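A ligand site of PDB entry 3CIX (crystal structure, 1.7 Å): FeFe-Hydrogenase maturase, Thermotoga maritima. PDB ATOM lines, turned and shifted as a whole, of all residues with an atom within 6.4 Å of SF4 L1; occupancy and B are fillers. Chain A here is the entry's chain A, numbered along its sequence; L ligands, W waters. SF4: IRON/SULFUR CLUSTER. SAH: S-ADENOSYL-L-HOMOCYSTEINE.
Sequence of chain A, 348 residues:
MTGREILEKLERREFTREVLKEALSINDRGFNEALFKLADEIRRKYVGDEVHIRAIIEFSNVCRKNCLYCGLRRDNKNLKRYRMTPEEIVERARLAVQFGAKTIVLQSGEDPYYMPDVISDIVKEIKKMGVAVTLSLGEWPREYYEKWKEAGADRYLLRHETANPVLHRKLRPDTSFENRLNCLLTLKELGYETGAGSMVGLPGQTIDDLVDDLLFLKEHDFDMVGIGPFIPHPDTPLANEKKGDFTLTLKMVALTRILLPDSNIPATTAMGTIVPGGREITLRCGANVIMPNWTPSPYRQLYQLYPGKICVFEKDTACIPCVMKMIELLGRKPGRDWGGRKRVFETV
The side-chain sulfur of Cys 63 is bound to an iron atom (FE3) of SF4 L1 (2.3 Å).
An iron atom (FE4) of SF4 L1 is bound by the side-chain sulfur (SG) of Cys 70 (2.3 Å).
A sulfur (S2) of SF4 L1 lies close to the backbone NH of Cys 67.
The side-chain sulfur (SG) of Cys 67 is bound to an iron atom (FE1) of SF4 L1.
The backbone carbonyl oxygen of Tyr 69 lies within hydrogen-bond range of a nitrogen (N6) of SAH L2.
The backbone carbonyl oxygen (O) of Ser 108 sits close to a nitrogen (N) of SAH L2, at 3.1 Å.
The side-chain carboxylate (OE2) of Glu 161 sits at hydrogen-bond distance from an oxygen (O3') of SAH L2, 2.6 Å away.
NH2 of Arg 180 lies within salt-bridge range of OXT of SAH L2 (3.0 Å).
O of SAH L2 binds FE2 of SF4 L1, at 2.3 Å.
The side-chain sulfur (SG) of Cys 63 lies close to the backbone NH (N) of Lys 65, at 3.3 Å.
The backbone NH of Glu 110 sits close to the side-chain sulfur of Cys 63 (3.3 Å).
SG of Cys 70 sits close to N of Leu 72, at 3.4 Å.
O of Cys 67 is in hydrogen-bond range of NE of Arg 73 (2.9 Å).
SG of Cys 67 lies close to NE of Arg 172 (3.6 Å).
The guanidinium group (NE) of Arg 172 sits at hydrogen-bond distance from the side-chain hydroxyl (OH) of Tyr 69, at 3.0 Å.
NZ of Lys 65 lies within salt-bridge range of OE1 of Glu 110 (2.7 Å).
The backbone NH of Arg 74 is in hydrogen-bond range of the backbone carbonyl oxygen of Lys 65, at 2.9 Å.
Merely in contact with SF4 L1: Gly 109 (3.7 Å), Tyr 69 (3.8 Å), Arg 73 (3.8 Å) and Lys 65 (3.8 Å).
Hydrophobic or aromatic side chains that line SF4 L1: Tyr 69.
Within 4 Å of SF4 L1: Cys 63, Lys 65, Cys 67, Tyr 69, Cys 70, Arg 73 and Gly 109.
The nearest printed residue that does not touch SF4 L1 is Glu 110 (4.004 Å).
Water W2 lies within hydrogen-bond range of the side-chain carboxylate (OE2) of Glu 161 (2.7 Å), the side-chain hydroxyl (OH) of Tyr 69 (2.8 Å), the guanidinium group (NE) of Arg 172 (3.1 Å) and a sulfur (S3) of SF4 L1 (3.3 Å).
Water W1 lies within hydrogen-bond range of OE2 of Glu 110 (2.6 Å), NH1 of Arg 180 (2.8 Å), NH2 of Arg 172 (3.3 Å) and S4 of SF4 L1 (3.3 Å).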
ATOM      1  N   VAL A  62       2.446  11.003  20.404  1.00  0.00           N
ATOM      2  CA  VAL A  62       2.480  10.824  21.859  1.00  0.00           C
ATOM      3  C   VAL A  62       1.826  12.005  22.550  1.00  0.00           C
ATOM      4  O   VAL A  62       2.153  13.167  22.255  1.00  0.00           O
ATOM      5  CB  VAL A  62       3.907  10.568  22.355  1.00  0.00           C
ATOM      6  CG1 VAL A  62       3.979  10.492  23.923  1.00  0.00           C
ATOM      7  CG2 VAL A  62       4.448   9.316  21.698  1.00  0.00           C
ATOM      8  N   CYS A  63       0.904  11.747  23.472  1.00  0.00           N
ATOM      9  CA  CYS A  63       0.291  12.838  24.237  1.00  0.00           C
ATOM     10  C   CYS A  63       0.075  12.467  25.684  1.00  0.00           C
ATOM     11  O   CYS A  63      -0.344  11.350  25.997  1.00  0.00           O
ATOM     12  CB  CYS A  63      -1.020  13.313  23.628  1.00  0.00           C
ATOM     13  SG  CYS A  63      -1.544  14.920  24.313  1.00  0.00           S
ATOM     14  N   ARG A  64       0.355  13.436  26.541  1.00  0.00           N
ATOM     15  CA  ARG A  64       0.164  13.346  27.982  1.00  0.00           C
ATOM     16  C   ARG A  64      -1.256  13.739  28.448  1.00  0.00           C
ATOM     17  O   ARG A  64      -1.641  13.446  29.600  1.00  0.00           O
ATOM     18  CB  ARG A  64       1.176  14.244  28.696  1.00  0.00           C
ATOM     19  CG  ARG A  64       0.893  15.747  28.612  1.00  0.00           C
ATOM     20  CD  ARG A  64       2.031  16.552  29.135  1.00  0.00           C
ATOM     21  NE  ARG A  64       1.851  17.966  28.899  1.00  0.00           N
ATOM     22  CZ  ARG A  64       2.475  18.951  29.538  1.00  0.00           C
ATOM     23  NH1 ARG A  64       3.382  18.713  30.476  1.00  0.00           N
ATOM     24  NH2 ARG A  64       2.199  20.222  29.217  1.00  0.00           N
ATOM     25  N   LYS A  65      -1.997  14.450  27.590  1.00  0.00           N
ATOM     26  CA  LYS A  65      -3.340  14.913  27.912  1.00  0.00           C
ATOM     27  C   LYS A  65      -4.415  13.920  27.460  1.00  0.00           C
ATOM     28  O   LYS A  65      -4.110  12.958  26.752  1.00  0.00           O
ATOM     29  CB  LYS A  65      -3.571  16.309  27.350  1.00  0.00           C
ATOM     30  CG  LYS A  65      -3.002  17.434  28.215  1.00  0.00           C
ATOM     31  CD  LYS A  65      -3.349  18.797  27.725  1.00  0.00           C
ATOM     32  CE  LYS A  65      -3.013  19.923  28.704  1.00  0.00           C
ATOM     33  NZ  LYS A  65      -1.614  20.015  29.158  1.00  0.00           N
ATOM     34  N   ASN A  66      -5.656  14.167  27.917  1.00  0.00           N
ATOM     35  CA  ASN A  66      -6.725  13.188  27.795  1.00  0.00           C
ATOM     36  C   ASN A  66      -8.002  13.833  27.281  1.00  0.00           C
ATOM     37  O   ASN A  66      -9.101  13.423  27.647  1.00  0.00           O
ATOM     38  CB  ASN A  66      -6.943  12.461  29.151  1.00  0.00           C
ATOM     39  CG  ASN A  66      -7.421  11.020  29.000  1.00  0.00           C
ATOM     40  OD1 ASN A  66      -7.211  10.384  27.994  1.00  0.00           O
ATOM     41  ND2 ASN A  66      -8.027  10.484  30.072  1.00  0.00           N
ATOM     42  N   CYS A  67      -7.872  14.827  26.402  1.00  0.00           N
ATOM     43  CA  CYS A  67      -9.026  15.547  25.814  1.00  0.00           C
ATOM     44  C   CYS A  67     -10.060  14.541  25.312  1.00  0.00           C
ATOM     45  O   CYS A  67      -9.713  13.575  24.665  1.00  0.00           O
ATOM     46  CB  CYS A  67      -8.549  16.489  24.690  1.00  0.00           C
ATOM     47  SG  CYS A  67      -7.284  17.642  25.303  1.00  0.00           S
ATOM     48  N   LEU A  68     -11.334  14.749  25.663  1.00  0.00           N
ATOM     49  CA  LEU A  68     -12.360  13.718  25.423  1.00  0.00           C
ATOM     50  C   LEU A  68     -12.671  13.515  23.942  1.00  0.00           C
ATOM     51  O   LEU A  68     -13.095  12.442  23.537  1.00  0.00           O
ATOM     52  CB  LEU A  68     -13.654  14.060  26.175  1.00  0.00           C
ATOM     53  CG  LEU A  68     -13.822  13.526  27.618  1.00  0.00           C
ATOM     54  CD1 LEU A  68     -12.660  13.936  28.483  1.00  0.00           C
ATOM     55  CD2 LEU A  68     -15.138  14.049  28.199  1.00  0.00           C
ATOM     56  N   TYR A  69     -12.407  14.545  23.133  1.00  0.00           N
ATOM     57  CA  TYR A  69     -12.707  14.477  21.688  1.00  0.00           C
ATOM     58  C   TYR A  69     -11.589  13.858  20.827  1.00  0.00           C
ATOM     59  O   TYR A  69     -11.827  13.466  19.674  1.00  0.00           O
ATOM     60  CB  TYR A  69     -12.999  15.886  21.164  1.00  0.00           C
ATOM     61  CG  TYR A  69     -12.035  16.924  21.624  1.00  0.00           C
ATOM     62  CD1 TYR A  69     -10.779  17.075  21.009  1.00  0.00           C
ATOM     63  CD2 TYR A  69     -12.346  17.771  22.706  1.00  0.00           C
ATOM     64  CE1 TYR A  69      -9.896  18.046  21.460  1.00  0.00           C
ATOM     65  CE2 TYR A  69     -11.453  18.723  23.150  1.00  0.00           C
ATOM     66  CZ  TYR A  69     -10.239  18.864  22.502  1.00  0.00           C
ATOM     67  OH  TYR A  69      -9.358  19.811  22.957  1.00  0.00           O
ATOM     68  N   CYS A  70     -10.383  13.768  21.374  1.00  0.00           N
ATOM     69  CA  CYS A  70      -9.186  13.560  20.560  1.00  0.00           C
ATOM     70  C   CYS A  70      -8.725  12.110  20.523  1.00  0.00           C
ATOM     71  O   CYS A  70      -8.585  11.465  21.583  1.00  0.00           O
ATOM     72  CB  CYS A  70      -8.053  14.424  21.088  1.00  0.00           C
ATOM     73  SG  CYS A  70      -6.603  14.362  20.017  1.00  0.00           S
ATOM     74  N   GLY A  71      -8.471  11.599  19.319  1.00  0.00           N
ATOM     75  CA  GLY A  71      -7.962  10.261  19.128  1.00  0.00           C
ATOM     76  C   GLY A  71      -6.562  10.008  19.675  1.00  0.00           C
ATOM     77  O   GLY A  71      -6.196   8.860  19.919  1.00  0.00           O
ATOM     78  N   LEU A  72      -5.766  11.063  19.895  1.00  0.00           N
ATOM     79  CA  LEU A  72      -4.428  10.900  20.487  1.00  0.00           C
ATOM     80  C   LEU A  72      -4.458  10.942  22.035  1.00  0.00           C
ATOM     81  O   LEU A  72      -3.425  10.863  22.666  1.00  0.00           O
ATOM     82  CB  LEU A  72      -3.425  11.952  19.945  1.00  0.00           C
ATOM     83  CG  LEU A  72      -3.305  12.119  18.436  1.00  0.00           C
ATOM     84  CD1 LEU A  72      -2.062  13.022  18.118  1.00  0.00           C
ATOM     85  CD2 LEU A  72      -3.261  10.836  17.676  1.00  0.00           C
ATOM     86  N   ARG A  73      -5.658  11.077  22.645  1.00  0.00           N
ATOM     87  CA  ARG A  73      -5.778  11.140  24.116  1.00  0.00           C
ATOM     88  C   ARG A  73      -5.011   9.969  24.785  1.00  0.00           C
ATOM     89  O   ARG A  73      -4.978   8.853  24.256  1.00  0.00           O
ATOM     90  CB  ARG A  73      -7.246  11.150  24.587  1.00  0.00           C
ATOM     91  CG  ARG A  73      -8.056   9.903  24.231  1.00  0.00           C
ATOM     92  CD  ARG A  73      -9.559  10.157  24.396  1.00  0.00           C
ATOM     93  NE  ARG A  73      -9.905  10.814  25.664  1.00  0.00           N
ATOM     94  CZ  ARG A  73     -10.264  10.193  26.793  1.00  0.00           C
ATOM     95  NH1 ARG A  73     -10.275   8.887  26.856  1.00  0.00           N
ATOM     96  NH2 ARG A  73     -10.538  10.872  27.883  1.00  0.00           N
ATOM     97  N   ARG A  74      -4.412  10.239  25.923  1.00  0.00           N
ATOM     98  CA  ARG A  74      -3.508   9.272  26.504  1.00  0.00           C
ATOM     99  C   ARG A  74      -4.177   7.939  26.843  1.00  0.00           C
ATOM    100  O   ARG A  74      -3.523   6.911  26.742  1.00  0.00           O
ATOM    101  CB  ARG A  74      -2.766   9.821  27.743  1.00  0.00           C
ATOM    102  CG  ARG A  74      -3.634  10.174  28.893  1.00  0.00           C
ATOM    103  CD  ARG A  74      -2.830  10.335  30.200  1.00  0.00           C
ATOM    104  NE  ARG A  74      -3.832  10.514  31.253  1.00  0.00           N
ATOM    105  CZ  ARG A  74      -4.328  11.682  31.628  1.00  0.00           C
ATOM    106  NH1 ARG A  74      -3.898  12.833  31.131  1.00  0.00           N
ATOM    107  NH2 ARG A  74      -5.299  11.703  32.528  1.00  0.00           N
ATOM    108  N   SER A 108       2.319  18.285  17.083  1.00  0.00           N
ATOM    109  CA  SER A 108       2.386  17.004  17.778  1.00  0.00           C
ATOM    110  C   SER A 108       1.351  16.923  18.873  1.00  0.00           C
ATOM    111  O   SER A 108       0.727  17.928  19.278  1.00  0.00           O
ATOM    112  CB  SER A 108       3.792  16.816  18.362  1.00  0.00           C
ATOM    113  OG  SER A 108       4.067  17.846  19.311  1.00  0.00           O
ATOM    114  N   GLY A 109       1.205  15.725  19.432  1.00  0.00           N
ATOM    115  CA  GLY A 109       0.571  15.619  20.748  1.00  0.00           C
ATOM    116  C   GLY A 109       1.483  16.308  21.755  1.00  0.00           C
ATOM    117  O   GLY A 109       2.604  16.673  21.426  1.00  0.00           O
ATOM    118  N   GLU A 110       0.998  16.520  22.966  1.00  0.00           N
ATOM    119  CA  GLU A 110       1.844  17.042  24.030  1.00  0.00           C
ATOM    120  C   GLU A 110       2.786  15.944  24.513  1.00  0.00           C
ATOM    121  O   GLU A 110       2.518  15.238  25.525  1.00  0.00           O
ATOM    122  CB  GLU A 110       1.011  17.626  25.179  1.00  0.00           C
ATOM    123  CG  GLU A 110       0.267  18.950  24.805  1.00  0.00           C
ATOM    124  CD  GLU A 110      -0.259  19.713  26.027  1.00  0.00           C
ATOM    125  OE1 GLU A 110       0.065  19.310  27.187  1.00  0.00           O
ATOM    126  OE2 GLU A 110      -1.001  20.716  25.829  1.00  0.00           O
ATOM    127  N   GLY A 138       0.796  22.497  21.784  1.00  0.00           N
ATOM    128  CA  GLY A 138      -0.008  22.533  23.000  1.00  0.00           C
ATOM    129  C   GLY A 138       0.485  23.519  24.083  1.00  0.00           C
ATOM    130  O   GLY A 138       1.114  24.527  23.793  1.00  0.00           O
ATOM    131  N   GLU A 161     -10.398  26.239  21.361  1.00  0.00           N
ATOM    132  CA  GLU A 161     -11.292  25.052  21.384  1.00  0.00           C
ATOM    133  C   GLU A 161     -12.756  25.402  21.668  1.00  0.00           C
ATOM    134  O   GLU A 161     -13.640  25.088  20.868  1.00  0.00           O
ATOM    135  CB  GLU A 161     -10.821  23.964  22.350  1.00  0.00           C
ATOM    136  CG  GLU A 161      -9.306  23.624  22.238  1.00  0.00           C
ATOM    137  CD  GLU A 161      -8.891  23.034  20.897  1.00  0.00           C
ATOM    138  OE1 GLU A 161      -9.672  23.010  19.914  1.00  0.00           O
ATOM    139  OE2 GLU A 161      -7.713  22.579  20.844  1.00  0.00           O
ATOM    140  N   ARG A 172     -11.613  18.948  28.472  1.00  0.00           N
ATOM    141  CA  ARG A 172     -10.163  18.997  28.555  1.00  0.00           C
ATOM    142  C   ARG A 172      -9.787  18.914  30.047  1.00  0.00           C
ATOM    143  O   ARG A 172      -9.396  19.913  30.656  1.00  0.00           O
ATOM    144  CB  ARG A 172      -9.646  20.253  27.861  1.00  0.00           C
ATOM    145  CG  ARG A 172     -10.227  20.450  26.448  1.00  0.00           C
ATOM    146  CD  ARG A 172      -9.490  21.530  25.636  1.00  0.00           C
ATOM    147  NE  ARG A 172      -8.116  21.104  25.391  1.00  0.00           N
ATOM    148  CZ  ARG A 172      -7.035  21.699  25.882  1.00  0.00           C
ATOM    149  NH1 ARG A 172      -7.139  22.825  26.577  1.00  0.00           N
ATOM    150  NH2 ARG A 172      -5.840  21.143  25.678  1.00  0.00           N
ATOM    151  N   ARG A 180      -5.597  28.029  28.970  1.00  0.00           N
ATOM    152  CA  ARG A 180      -5.469  28.147  27.509  1.00  0.00           C
ATOM    153  C   ARG A 180      -5.326  29.614  27.112  1.00  0.00           C
ATOM    154  O   ARG A 180      -4.447  29.993  26.321  1.00  0.00           O
ATOM    155  CB  ARG A 180      -6.695  27.533  26.837  1.00  0.00           C
ATOM    156  CG  ARG A 180      -6.535  27.202  25.359  1.00  0.00           C
ATOM    157  CD  ARG A 180      -5.771  25.913  25.187  1.00  0.00           C
ATOM    158  NE  ARG A 180      -5.768  25.430  23.826  1.00  0.00           N
ATOM    159  CZ  ARG A 180      -5.091  24.347  23.434  1.00  0.00           C
ATOM    160  NH1 ARG A 180      -4.327  23.685  24.294  1.00  0.00           N
ATOM    161  NH2 ARG A 180      -5.122  23.943  22.159  1.00  0.00           N
ATOM    162  N   TYR A 303      -1.580   9.424  12.831  1.00  0.00           N
ATOM    163  CA  TYR A 303      -1.916  10.695  13.443  1.00  0.00           C
ATOM    164  C   TYR A 303      -3.412  10.941  13.266  1.00  0.00           C
ATOM    165  O   TYR A 303      -3.823  11.678  12.392  1.00  0.00           O
ATOM    166  CB  TYR A 303      -1.044  11.813  12.862  1.00  0.00           C
ATOM    167  CG  TYR A 303      -1.069  13.066  13.689  1.00  0.00           C
ATOM    168  CD1 TYR A 303      -0.237  13.221  14.812  1.00  0.00           C
ATOM    169  CD2 TYR A 303      -1.942  14.103  13.377  1.00  0.00           C
ATOM    170  CE1 TYR A 303      -0.212  14.395  15.534  1.00  0.00           C
ATOM    171  CE2 TYR A 303      -1.937  15.284  14.124  1.00  0.00           C
ATOM    172  CZ  TYR A 303      -1.083  15.410  15.213  1.00  0.00           C
ATOM    173  OH  TYR A 303      -1.049  16.572  15.965  1.00  0.00           O
ATOM    174  N   LEU A 305      -6.326  12.295  14.937  1.00  0.00           N
ATOM    175  CA  LEU A 305      -7.079  13.158  15.882  1.00  0.00           C
ATOM    176  C   LEU A 305      -8.550  12.791  15.766  1.00  0.00           C
ATOM    177  O   LEU A 305      -9.265  12.709  16.759  1.00  0.00           O
ATOM    178  CB  LEU A 305      -6.894  14.652  15.577  1.00  0.00           C
ATOM    179  CG  LEU A 305      -5.472  15.212  15.481  1.00  0.00           C
ATOM    180  CD1 LEU A 305      -5.480  16.627  14.855  1.00  0.00           C
ATOM    181  CD2 LEU A 305      -4.823  15.229  16.841  1.00  0.00           C
HETATM  182 FE1  SF4 L   1      -5.621  17.164  23.611  1.00  0.00          FE
HETATM  183 FE2  SF4 L   1      -3.816  18.085  21.552  1.00  0.00          FE
HETATM  184 FE3  SF4 L   1      -3.315  15.761  23.194  1.00  0.00          FE
HETATM  185 FE4  SF4 L   1      -5.291  15.682  21.355  1.00  0.00          FE
HETATM  186  S1  SF4 L   1      -3.066  15.944  20.886  1.00  0.00           S
HETATM  187  S2  SF4 L   1      -5.372  14.876  23.544  1.00  0.00           S
HETATM  188  S3  SF4 L   1      -6.133  17.853  21.435  1.00  0.00           S
HETATM  189  S4  SF4 L   1      -3.500  17.953  23.886  1.00  0.00           S
HETATM  190  N   SAH L   2      -1.695  18.841  21.001  1.00  0.00           N
HETATM  191  CA  SAH L   2      -1.816  20.207  20.374  1.00  0.00           C
HETATM  192  CB  SAH L   2      -1.743  20.138  18.833  1.00  0.00           C
HETATM  193  CG  SAH L   2      -2.473  18.984  18.154  1.00  0.00           C
HETATM  194  SD  SAH L   2      -4.272  18.910  18.323  1.00  0.00           S
HETATM  195  C   SAH L   2      -3.048  20.959  20.856  1.00  0.00           C
HETATM  196  O   SAH L   2      -3.920  20.381  21.485  1.00  0.00           O
HETATM  197  OXT SAH L   2      -3.156  22.189  20.650  1.00  0.00           O
HETATM  198  C5' SAH L   2      -4.791  19.957  16.891  1.00  0.00           C
HETATM  199  C4' SAH L   2      -6.281  20.399  16.828  1.00  0.00           C
HETATM  200  O4' SAH L   2      -7.120  19.353  16.294  1.00  0.00           O
HETATM  201  C3' SAH L   2      -6.958  20.759  18.139  1.00  0.00           C
HETATM  202  O3' SAH L   2      -6.689  22.081  18.552  1.00  0.00           O
HETATM  203  C2' SAH L   2      -8.436  20.450  17.910  1.00  0.00           C
HETATM  204  O2' SAH L   2      -9.209  21.593  17.688  1.00  0.00           O
HETATM  205  C1' SAH L   2      -8.445  19.540  16.661  1.00  0.00           C
HETATM  206  N9  SAH L   2      -9.106  18.272  16.993  1.00  0.00           N
HETATM  207  C8  SAH L   2      -8.740  17.322  17.917  1.00  0.00           C
HETATM  208  N7  SAH L   2      -9.644  16.331  17.912  1.00  0.00           N
HETATM  209  C5  SAH L   2     -10.627  16.645  17.007  1.00  0.00           C
HETATM  210  C6  SAH L   2     -11.768  15.993  16.584  1.00  0.00           C
HETATM  211  N6  SAH L   2     -12.209  14.822  17.107  1.00  0.00           N
HETATM  212  N1  SAH L   2     -12.517  16.599  15.592  1.00  0.00           N
HETATM  213  C2  SAH L   2     -12.147  17.785  15.011  1.00  0.00           C
HETATM  214  N3  SAH L   2     -11.014  18.417  15.416  1.00  0.00           N
HETATM  215  C4  SAH L   2     -10.260  17.836  16.390  1.00  0.00           C
HETATM  216  O   HOH W   1      -2.966  21.198  24.130  1.00  0.00           O
HETATM  217  O   HOH W   2      -6.755  20.832  22.650  1.00  0.00           O
